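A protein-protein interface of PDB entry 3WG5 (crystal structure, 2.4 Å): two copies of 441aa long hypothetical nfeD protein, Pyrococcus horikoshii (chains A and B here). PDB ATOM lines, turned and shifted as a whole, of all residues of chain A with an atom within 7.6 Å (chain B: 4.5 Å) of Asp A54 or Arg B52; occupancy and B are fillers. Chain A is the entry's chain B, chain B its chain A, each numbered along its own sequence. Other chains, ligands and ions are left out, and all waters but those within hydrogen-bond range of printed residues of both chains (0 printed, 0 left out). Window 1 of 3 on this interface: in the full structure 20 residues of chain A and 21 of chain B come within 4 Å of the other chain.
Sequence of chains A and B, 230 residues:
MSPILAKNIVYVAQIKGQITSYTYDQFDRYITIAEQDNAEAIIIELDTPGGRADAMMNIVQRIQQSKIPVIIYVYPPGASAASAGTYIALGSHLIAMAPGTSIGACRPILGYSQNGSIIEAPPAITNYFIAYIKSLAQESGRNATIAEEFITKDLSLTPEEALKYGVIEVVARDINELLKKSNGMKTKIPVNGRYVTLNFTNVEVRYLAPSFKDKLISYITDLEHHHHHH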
ATOM      1  N   ILE A  19     -20.671  10.539 -29.989  1.00  0.00           N
ATOM      2  CA  ILE A  19     -20.129  11.207 -28.807  1.00  0.00           C
ATOM      3  C   ILE A  19     -18.637  11.468 -28.995  1.00  0.00           C
ATOM      4  O   ILE A  19     -17.854  10.533 -29.107  1.00  0.00           O
ATOM      5  CB  ILE A  19     -20.359  10.406 -27.495  1.00  0.00           C
ATOM      6  CG1 ILE A  19     -21.842  10.046 -27.294  1.00  0.00           C
ATOM      7  CG2 ILE A  19     -19.810  11.183 -26.310  1.00  0.00           C
ATOM      8  CD1 ILE A  19     -22.809  11.252 -27.215  1.00  0.00           C
ATOM      9  N   THR A  20     -18.265  12.747 -29.040  1.00  0.00           N
ATOM     10  CA  THR A  20     -16.871  13.172 -29.193  1.00  0.00           C
ATOM     11  C   THR A  20     -16.564  14.325 -28.225  1.00  0.00           C
ATOM     12  O   THR A  20     -17.395  14.688 -27.391  1.00  0.00           O
ATOM     13  CB  THR A  20     -16.568  13.681 -30.647  1.00  0.00           C
ATOM     14  OG1 THR A  20     -17.180  14.956 -30.821  1.00  0.00           O
ATOM     15  CG2 THR A  20     -17.084  12.730 -31.724  1.00  0.00           C
ATOM     16  N   SER A  21     -15.367  14.895 -28.362  1.00  0.00           N
ATOM     17  CA  SER A  21     -14.932  16.109 -27.661  1.00  0.00           C
ATOM     18  C   SER A  21     -15.872  17.294 -27.817  1.00  0.00           C
ATOM     19  O   SER A  21     -16.045  18.076 -26.876  1.00  0.00           O
ATOM     20  CB  SER A  21     -13.555  16.534 -28.170  1.00  0.00           C
ATOM     21  OG  SER A  21     -12.595  15.557 -27.834  1.00  0.00           O
ATOM     22  N   TYR A  24     -18.777  16.670 -25.515  1.00  0.00           N
ATOM     23  CA  TYR A  24     -18.410  17.108 -24.172  1.00  0.00           C
ATOM     24  C   TYR A  24     -18.621  18.616 -24.041  1.00  0.00           C
ATOM     25  O   TYR A  24     -19.251  19.093 -23.096  1.00  0.00           O
ATOM     26  CB  TYR A  24     -16.952  16.759 -23.803  1.00  0.00           C
ATOM     27  CG  TYR A  24     -16.580  17.430 -22.501  1.00  0.00           C
ATOM     28  CD1 TYR A  24     -16.938  16.854 -21.282  1.00  0.00           C
ATOM     29  CD2 TYR A  24     -15.967  18.694 -22.486  1.00  0.00           C
ATOM     30  CE1 TYR A  24     -16.645  17.476 -20.083  1.00  0.00           C
ATOM     31  CE2 TYR A  24     -15.678  19.334 -21.287  1.00  0.00           C
ATOM     32  CZ  TYR A  24     -16.019  18.715 -20.085  1.00  0.00           C
ATOM     33  OH  TYR A  24     -15.751  19.326 -18.879  1.00  0.00           O
ATOM     34  N   GLY A  51     -19.893   6.478 -29.759  1.00  0.00           N
ATOM     35  CA  GLY A  51     -18.824   7.467 -29.757  1.00  0.00           C
ATOM     36  C   GLY A  51     -17.625   7.079 -28.927  1.00  0.00           C
ATOM     37  O   GLY A  51     -17.449   5.908 -28.602  1.00  0.00           O
ATOM     38  N   ARG A  52     -16.810   8.070 -28.569  1.00  0.00           N
ATOM     39  CA  ARG A  52     -15.527   7.810 -27.921  1.00  0.00           C
ATOM     40  C   ARG A  52     -15.618   7.690 -26.385  1.00  0.00           C
ATOM     41  O   ARG A  52     -16.372   8.423 -25.723  1.00  0.00           O
ATOM     42  CB  ARG A  52     -14.469   8.857 -28.335  1.00  0.00           C
ATOM     43  CG  ARG A  52     -14.331   9.184 -29.868  1.00  0.00           C
ATOM     44  CD  ARG A  52     -14.445   7.976 -30.862  1.00  0.00           C
ATOM     45  NE  ARG A  52     -13.290   7.065 -30.873  1.00  0.00           N
ATOM     46  CZ  ARG A  52     -12.873   6.361 -31.932  1.00  0.00           C
ATOM     47  NH1 ARG A  52     -13.484   6.459 -33.108  1.00  0.00           N
ATOM     48  NH2 ARG A  52     -11.820   5.562 -31.822  1.00  0.00           N
ATOM     49  N   ALA A  53     -14.822   6.777 -25.837  1.00  0.00           N
ATOM     50  CA  ALA A  53     -14.844   6.432 -24.416  1.00  0.00           C
ATOM     51  C   ALA A  53     -14.434   7.576 -23.505  1.00  0.00           C
ATOM     52  O   ALA A  53     -15.101   7.828 -22.495  1.00  0.00           O
ATOM     53  CB  ALA A  53     -13.977   5.221 -24.153  1.00  0.00           C
ATOM     54  N   ASP A  54     -13.354   8.273 -23.862  1.00  0.00           N
ATOM     55  CA  ASP A  54     -12.825   9.334 -23.011  1.00  0.00           C
ATOM     56  C   ASP A  54     -13.796  10.497 -22.897  1.00  0.00           C
ATOM     57  O   ASP A  54     -13.975  11.062 -21.810  1.00  0.00           O
ATOM     58  CB  ASP A  54     -11.402   9.779 -23.428  1.00  0.00           C
ATOM     59  CG  ASP A  54     -11.340  10.477 -24.807  1.00  0.00           C
ATOM     60  OD1 ASP A  54     -10.611  11.490 -24.907  1.00  0.00           O
ATOM     61  OD2 ASP A  54     -11.969  10.009 -25.785  1.00  0.00           O
ATOM     62  N   ALA A  55     -14.446  10.829 -24.010  1.00  0.00           N
ATOM     63  CA  ALA A  55     -15.423  11.908 -24.017  1.00  0.00           C
ATOM     64  C   ALA A  55     -16.655  11.517 -23.211  1.00  0.00           C
ATOM     65  O   ALA A  55     -17.191  12.324 -22.469  1.00  0.00           O
ATOM     66  CB  ALA A  55     -15.803  12.291 -25.445  1.00  0.00           C
ATOM     67  N   MET A  56     -17.093  10.275 -23.381  1.00  0.00           N
ATOM     68  CA  MET A  56     -18.186   9.705 -22.611  1.00  0.00           C
ATOM     69  C   MET A  56     -17.910   9.805 -21.101  1.00  0.00           C
ATOM     70  O   MET A  56     -18.768  10.236 -20.335  1.00  0.00           O
ATOM     71  CB  MET A  56     -18.393   8.246 -23.030  1.00  0.00           C
ATOM     72  CG  MET A  56     -19.437   7.505 -22.244  1.00  0.00           C
ATOM     73  SD  MET A  56     -18.711   6.794 -20.769  1.00  0.00           S
ATOM     74  CE  MET A  56     -17.918   5.321 -21.443  1.00  0.00           C
ATOM     75  N   MET A  57     -16.704   9.419 -20.695  1.00  0.00           N
ATOM     76  CA  MET A  57     -16.320   9.454 -19.291  1.00  0.00           C
ATOM     77  C   MET A  57     -16.201  10.878 -18.781  1.00  0.00           C
ATOM     78  O   MET A  57     -16.540  11.149 -17.625  1.00  0.00           O
ATOM     79  CB  MET A  57     -15.025   8.680 -19.061  1.00  0.00           C
ATOM     80  CG  MET A  57     -15.210   7.191 -19.265  1.00  0.00           C
ATOM     81  SD  MET A  57     -13.660   6.288 -19.150  1.00  0.00           S
ATOM     82  CE  MET A  57     -14.285   4.625 -19.199  1.00  0.00           C
ATOM     83  N   ASN A  58     -15.736  11.780 -19.641  1.00  0.00           N
ATOM     84  CA  ASN A  58     -15.693  13.191 -19.303  1.00  0.00           C
ATOM     85  C   ASN A  58     -17.092  13.761 -19.144  1.00  0.00           C
ATOM     86  O   ASN A  58     -17.315  14.613 -18.289  1.00  0.00           O
ATOM     87  CB  ASN A  58     -14.904  13.996 -20.346  1.00  0.00           C
ATOM     88  CG  ASN A  58     -13.398  13.789 -20.239  1.00  0.00           C
ATOM     89  OD1 ASN A  58     -12.898  13.244 -19.263  1.00  0.00           O
ATOM     90  ND2 ASN A  58     -12.669  14.230 -21.256  1.00  0.00           N
ATOM     91  N   ILE A  59     -18.029  13.292 -19.968  1.00  0.00           N
ATOM     92  CA  ILE A  59     -19.419  13.732 -19.867  1.00  0.00           C
ATOM     93  C   ILE A  59     -20.067  13.205 -18.572  1.00  0.00           C
ATOM     94  O   ILE A  59     -20.722  13.960 -17.863  1.00  0.00           O
ATOM     95  CB  ILE A  59     -20.245  13.378 -21.131  1.00  0.00           C
ATOM     96  CG1 ILE A  59     -19.739  14.188 -22.331  1.00  0.00           C
ATOM     97  CG2 ILE A  59     -21.730  13.683 -20.920  1.00  0.00           C
ATOM     98  CD1 ILE A  59     -20.183  13.656 -23.666  1.00  0.00           C
ATOM     99  N   VAL A  60     -19.850  11.934 -18.247  1.00  0.00           N
ATOM    100  CA  VAL A  60     -20.372  11.382 -17.003  1.00  0.00           C
ATOM    101  C   VAL A  60     -19.836  12.191 -15.814  1.00  0.00           C
ATOM    102  O   VAL A  60     -20.589  12.561 -14.922  1.00  0.00           O
ATOM    103  CB  VAL A  60     -20.075   9.870 -16.880  1.00  0.00           C
ATOM    104  CG1 VAL A  60     -20.426   9.334 -15.488  1.00  0.00           C
ATOM    105  CG2 VAL A  60     -20.839   9.107 -17.952  1.00  0.00           C
ATOM    106  N   GLN A  61     -18.541  12.501 -15.858  1.00  0.00           N
ATOM    107  CA  GLN A  61     -17.854  13.282 -14.834  1.00  0.00           C
ATOM    108  C   GLN A  61     -18.411  14.712 -14.722  1.00  0.00           C
ATOM    109  O   GLN A  61     -18.592  15.231 -13.617  1.00  0.00           O
ATOM    110  CB  GLN A  61     -16.350  13.294 -15.130  1.00  0.00           C
ATOM    111  CG  GLN A  61     -15.471  13.992 -14.104  1.00  0.00           C
ATOM    112  CD  GLN A  61     -15.078  13.114 -12.927  1.00  0.00           C
ATOM    113  OE1 GLN A  61     -15.838  12.236 -12.497  1.00  0.00           O
ATOM    114  NE2 GLN A  61     -13.884  13.360 -12.384  1.00  0.00           N
ATOM    115  N   LEU A 110     -12.793  -2.307 -30.661  1.00  0.00           N
ATOM    116  CA  LEU A 110     -11.707  -1.391 -30.994  1.00  0.00           C
ATOM    117  C   LEU A 110     -12.136  -0.491 -32.148  1.00  0.00           C
ATOM    118  O   LEU A 110     -11.657   0.633 -32.264  1.00  0.00           O
ATOM    119  CB  LEU A 110     -10.405  -2.130 -31.303  1.00  0.00           C
ATOM    120  CG  LEU A 110      -9.658  -2.797 -30.142  1.00  0.00           C
ATOM    121  CD1 LEU A 110      -8.332  -3.358 -30.629  1.00  0.00           C
ATOM    122  CD2 LEU A 110      -9.412  -1.848 -28.991  1.00  0.00           C
ATOM    123  N   PHE A 129     -15.179  -2.219 -18.933  1.00  0.00           N
ATOM    124  CA  PHE A 129     -16.444  -1.522 -19.149  1.00  0.00           C
ATOM    125  C   PHE A 129     -17.618  -2.160 -18.433  1.00  0.00           C
ATOM    126  O   PHE A 129     -18.536  -1.451 -18.023  1.00  0.00           O
ATOM    127  CB  PHE A 129     -16.704  -1.246 -20.629  1.00  0.00           C
ATOM    128  CG  PHE A 129     -15.864  -0.130 -21.159  1.00  0.00           C
ATOM    129  CD1 PHE A 129     -14.610  -0.383 -21.698  1.00  0.00           C
ATOM    130  CD2 PHE A 129     -16.291   1.182 -21.040  1.00  0.00           C
ATOM    131  CE1 PHE A 129     -13.805   0.661 -22.151  1.00  0.00           C
ATOM    132  CE2 PHE A 129     -15.507   2.230 -21.492  1.00  0.00           C
ATOM    133  CZ  PHE A 129     -14.256   1.973 -22.052  1.00  0.00           C
ATOM    134  N   TYR A 132     -17.295  -0.673 -15.009  1.00  0.00           N
ATOM    135  CA  TYR A 132     -17.719   0.730 -15.097  1.00  0.00           C
ATOM    136  C   TYR A 132     -19.250   0.893 -15.198  1.00  0.00           C
ATOM    137  O   TYR A 132     -19.849   1.687 -14.464  1.00  0.00           O
ATOM    138  CB  TYR A 132     -17.014   1.418 -16.280  1.00  0.00           C
ATOM    139  CG  TYR A 132     -17.268   2.911 -16.404  1.00  0.00           C
ATOM    140  CD1 TYR A 132     -16.830   3.803 -15.419  1.00  0.00           C
ATOM    141  CD2 TYR A 132     -17.930   3.433 -17.520  1.00  0.00           C
ATOM    142  CE1 TYR A 132     -17.055   5.172 -15.538  1.00  0.00           C
ATOM    143  CE2 TYR A 132     -18.157   4.795 -17.655  1.00  0.00           C
ATOM    144  CZ  TYR A 132     -17.718   5.660 -16.662  1.00  0.00           C
ATOM    145  OH  TYR A 132     -17.947   7.014 -16.785  1.00  0.00           O
ATOM    146  N   ILE B  19      -4.722  11.332 -36.564  1.00  0.00           N
ATOM    147  CA  ILE B  19      -5.168  10.177 -37.319  1.00  0.00           C
ATOM    148  C   ILE B  19      -6.587   9.843 -36.864  1.00  0.00           C
ATOM    149  O   ILE B  19      -6.789   9.422 -35.725  1.00  0.00           O
ATOM    150  CB  ILE B  19      -4.211   8.969 -37.107  1.00  0.00           C
ATOM    151  CG1 ILE B  19      -2.771   9.304 -37.545  1.00  0.00           C
ATOM    152  CG2 ILE B  19      -4.756   7.727 -37.790  1.00  0.00           C
ATOM    153  CD1 ILE B  19      -2.643   9.915 -38.953  1.00  0.00           C
ATOM    154  N   GLY B  51      -3.490  10.119 -32.662  1.00  0.00           N
ATOM    155  CA  GLY B  51      -4.677   9.640 -33.341  1.00  0.00           C
ATOM    156  C   GLY B  51      -5.364   8.470 -32.683  1.00  0.00           C
ATOM    157  O   GLY B  51      -5.019   8.067 -31.572  1.00  0.00           O
ATOM    158  N   ARG B  52      -6.346   7.922 -33.386  1.00  0.00           N
ATOM    159  CA  ARG B  52      -7.160   6.837 -32.851  1.00  0.00           C
ATOM    160  C   ARG B  52      -6.692   5.453 -33.337  1.00  0.00           C
ATOM    161  O   ARG B  52      -6.307   5.279 -34.504  1.00  0.00           O
ATOM    162  CB  ARG B  52      -8.631   7.086 -33.190  1.00  0.00           C
ATOM    163  CG  ARG B  52      -9.187   8.426 -32.621  1.00  0.00           C
ATOM    164  CD  ARG B  52      -9.821   8.235 -31.231  1.00  0.00           C
ATOM    165  NE  ARG B  52     -10.089   9.495 -30.527  1.00  0.00           N
ATOM    166  CZ  ARG B  52     -10.683   9.595 -29.332  1.00  0.00           C
ATOM    167  NH1 ARG B  52     -10.876  10.790 -28.781  1.00  0.00           N
ATOM    168  NH2 ARG B  52     -11.086   8.507 -28.680  1.00  0.00           N
ATOM    169  N   ALA B  53      -6.718   4.481 -32.425  1.00  0.00           N
ATOM    170  CA  ALA B  53      -6.288   3.115 -32.712  1.00  0.00           C
ATOM    171  C   ALA B  53      -7.038   2.477 -33.887  1.00  0.00           C
ATOM    172  O   ALA B  53      -6.410   1.865 -34.764  1.00  0.00           O
ATOM    173  CB  ALA B  53      -6.409   2.252 -31.466  1.00  0.00           C
ATOM    174  N   ASP B  54      -8.360   2.633 -33.919  1.00  0.00           N
ATOM    175  CA  ASP B  54      -9.171   2.005 -34.970  1.00  0.00           C
ATOM    176  C   ASP B  54      -8.840   2.510 -36.383  1.00  0.00           C
ATOM    177  O   ASP B  54      -8.693   1.716 -37.316  1.00  0.00           O
ATOM    178  CB  ASP B  54     -10.690   2.056 -34.660  1.00  0.00           C
ATOM    179  CG  ASP B  54     -11.279   3.483 -34.646  1.00  0.00           C
ATOM    180  OD1 ASP B  54     -12.496   3.600 -34.915  1.00  0.00           O
ATOM    181  OD2 ASP B  54     -10.570   4.476 -34.367  1.00  0.00           O
ATOM    182  N   ALA B  55      -8.697   3.822 -36.534  1.00  0.00           N
ATOM    183  CA  ALA B  55      -8.299   4.397 -37.829  1.00  0.00           C
ATOM    184  C   ALA B  55      -6.876   3.967 -38.219  1.00  0.00           C
ATOM    185  O   ALA B  55      -6.623   3.602 -39.369  1.00  0.00           O
ATOM    186  CB  ALA B  55      -8.439   5.917 -37.819  1.00  0.00           C
ATOM    187  N   MET B  56      -5.966   4.017 -37.257  1.00  0.00           N
ATOM    188  CA  MET B  56      -4.598   3.526 -37.410  1.00  0.00           C
ATOM    189  C   MET B  56      -4.592   2.098 -37.976  1.00  0.00           C
ATOM    190  O   MET B  56      -3.938   1.835 -38.987  1.00  0.00           O
ATOM    191  CB  MET B  56      -3.886   3.592 -36.053  1.00  0.00           C
ATOM    192  CG  MET B  56      -2.478   3.065 -36.012  1.00  0.00           C
ATOM    193  SD  MET B  56      -2.446   1.321 -35.549  1.00  0.00           S
ATOM    194  CE  MET B  56      -2.793   1.457 -33.782  1.00  0.00           C
ATOM    195  N   ALA B  84      -0.064   7.080 -33.173  1.00  0.00           N
ATOM    196  CA  ALA B  84      -0.627   6.254 -34.266  1.00  0.00           C
ATOM    197  C   ALA B  84       0.185   6.247 -35.545  1.00  0.00           C
ATOM    198  O   ALA B  84       0.198   5.239 -36.262  1.00  0.00           O
ATOM    199  CB  ALA B  84      -2.071   6.651 -34.583  1.00  0.00           C
ATOM    200  N   LEU B 110      -6.448   5.501 -22.843  1.00  0.00           N
ATOM    201  CA  LEU B 110      -7.888   5.643 -22.932  1.00  0.00           C
ATOM    202  C   LEU B 110      -8.283   7.062 -23.331  1.00  0.00           C
ATOM    203  O   LEU B 110      -9.401   7.285 -23.785  1.00  0.00           O
ATOM    204  CB  LEU B 110      -8.567   5.231 -21.618  1.00  0.00           C
ATOM    205  CG  LEU B 110      -9.060   3.785 -21.512  1.00  0.00           C
ATOM    206  CD1 LEU B 110      -9.539   3.509 -20.096  1.00  0.00           C
ATOM    207  CD2 LEU B 110     -10.175   3.490 -22.521  1.00  0.00           C
ATOM    208  N   GLY B 111      -7.368   8.016 -23.167  1.00  0.00           N
ATOM    209  CA  GLY B 111      -7.615   9.386 -23.621  1.00  0.00           C
ATOM    210  C   GLY B 111      -7.294  10.471 -22.611  1.00  0.00           C
ATOM    211  O   GLY B 111      -6.364  10.336 -21.808  1.00  0.00           O
ATOM    212  N   TYR B 112      -8.074  11.543 -22.653  1.00  0.00           N
ATOM    213  CA  TYR B 112      -7.797  12.726 -21.848  1.00  0.00           C
ATOM    214  C   TYR B 112      -8.962  13.139 -20.950  1.00  0.00           C
ATOM    215  O   TYR B 112     -10.103  13.257 -21.406  1.00  0.00           O
ATOM    216  CB  TYR B 112      -7.371  13.897 -22.752  1.00  0.00           C
ATOM    217  CG  TYR B 112      -6.202  13.570 -23.673  1.00  0.00           C
ATOM    218  CD1 TYR B 112      -6.398  13.393 -25.046  1.00  0.00           C
ATOM    219  CD2 TYR B 112      -4.907  13.431 -23.171  1.00  0.00           C
ATOM    220  CE1 TYR B 112      -5.332  13.093 -25.897  1.00  0.00           C
ATOM    221  CE2 TYR B 112      -3.835  13.130 -24.013  1.00  0.00           C
ATOM    222  CZ  TYR B 112      -4.056  12.963 -25.375  1.00  0.00           C
ATOM    223  OH  TYR B 112      -2.999  12.663 -26.210  1.00  0.00           O
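The side-chain carboxylate (OD1) of Asp A54 sits at hydrogen-bond distance from the backbone NH (N) of Tyr B112 (3.4 Å). The guanidinium group (NH2) of Arg B52 sits close to the guanidinium group (NE) of Arg A52, 3.4 Å away. O of Tyr B112 is in hydrogen-bond range of ND2 of Asn A58. NH1 of Arg B52 is in salt-bridge range of OD2 of Asp A54. The side-chain carboxylate of Asp B54 is in salt-bridge range of the guanidinium group of Arg A52 (3.0 Å).
The backbone carbonyl oxygen of Ile A19 is in hydrogen-bond range of the backbone NH of Arg A52 (2.7 Å). The backbone NH (N) of Arg B52 lies within hydrogen-bond range of the backbone carbonyl oxygen (O) of Ile B19 (2.8 Å). The side-chain amide nitrogen (ND2) of Asn A58 lies close to the backbone carbonyl oxygen (O) of Asp A54 (3.5 Å).
Asp A54 touches Leu B110 (CB to O, 3.2 Å). Asp A54 touches Gly B111 (CB to CA, 3.8 Å). Asp B54 touches Leu A110 (CB to O, 2.9 Å).
Asp A54 touches four residues of chain B. Of the printed residues of chain B, Leu A110 touches Asp B54 (2.9 Å). Of the printed residues of chain A, Tyr B112 touches Asp A54 (3.4 Å) and Asn A58 (2.7 Å). The nearest residue of chain A that does not touch Arg B52 is Ala A53 (5.0 Å).
Of the 18 printed residues of chain A, 4 touch a printed residue of chain B. Printed residues of chain A that touch a printed residue of chain B: Arg A52, Asp A54, Asn A58 and Leu A110. Of the 11 printed residues of chain B, 5 touch a printed residue of chain A. Printed residues of chain B that touch a printed residue of chain A: Arg B52, Asp B54, Leu B110, Gly B111 and Tyr B112. Among the printed residues, Asp or Glu carboxylates within 4 Å of a Lys or Arg side-chain nitrogen of the other chain: Arg A52 with Asp B54 and Asp A54 with Arg B52.
Arg B52 touches its own counterpart, Arg A52. Arg A52 touches Asp B54, and with the chains exchanged Asp A54 touches Arg B52. Asp A54 touches Leu B110, and with the chains exchanged Leu A110 touches Asp B54. Of the 8 pairs that touch across the chains among the printed residues, 5 have their exchanged pair printed and touching as well.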
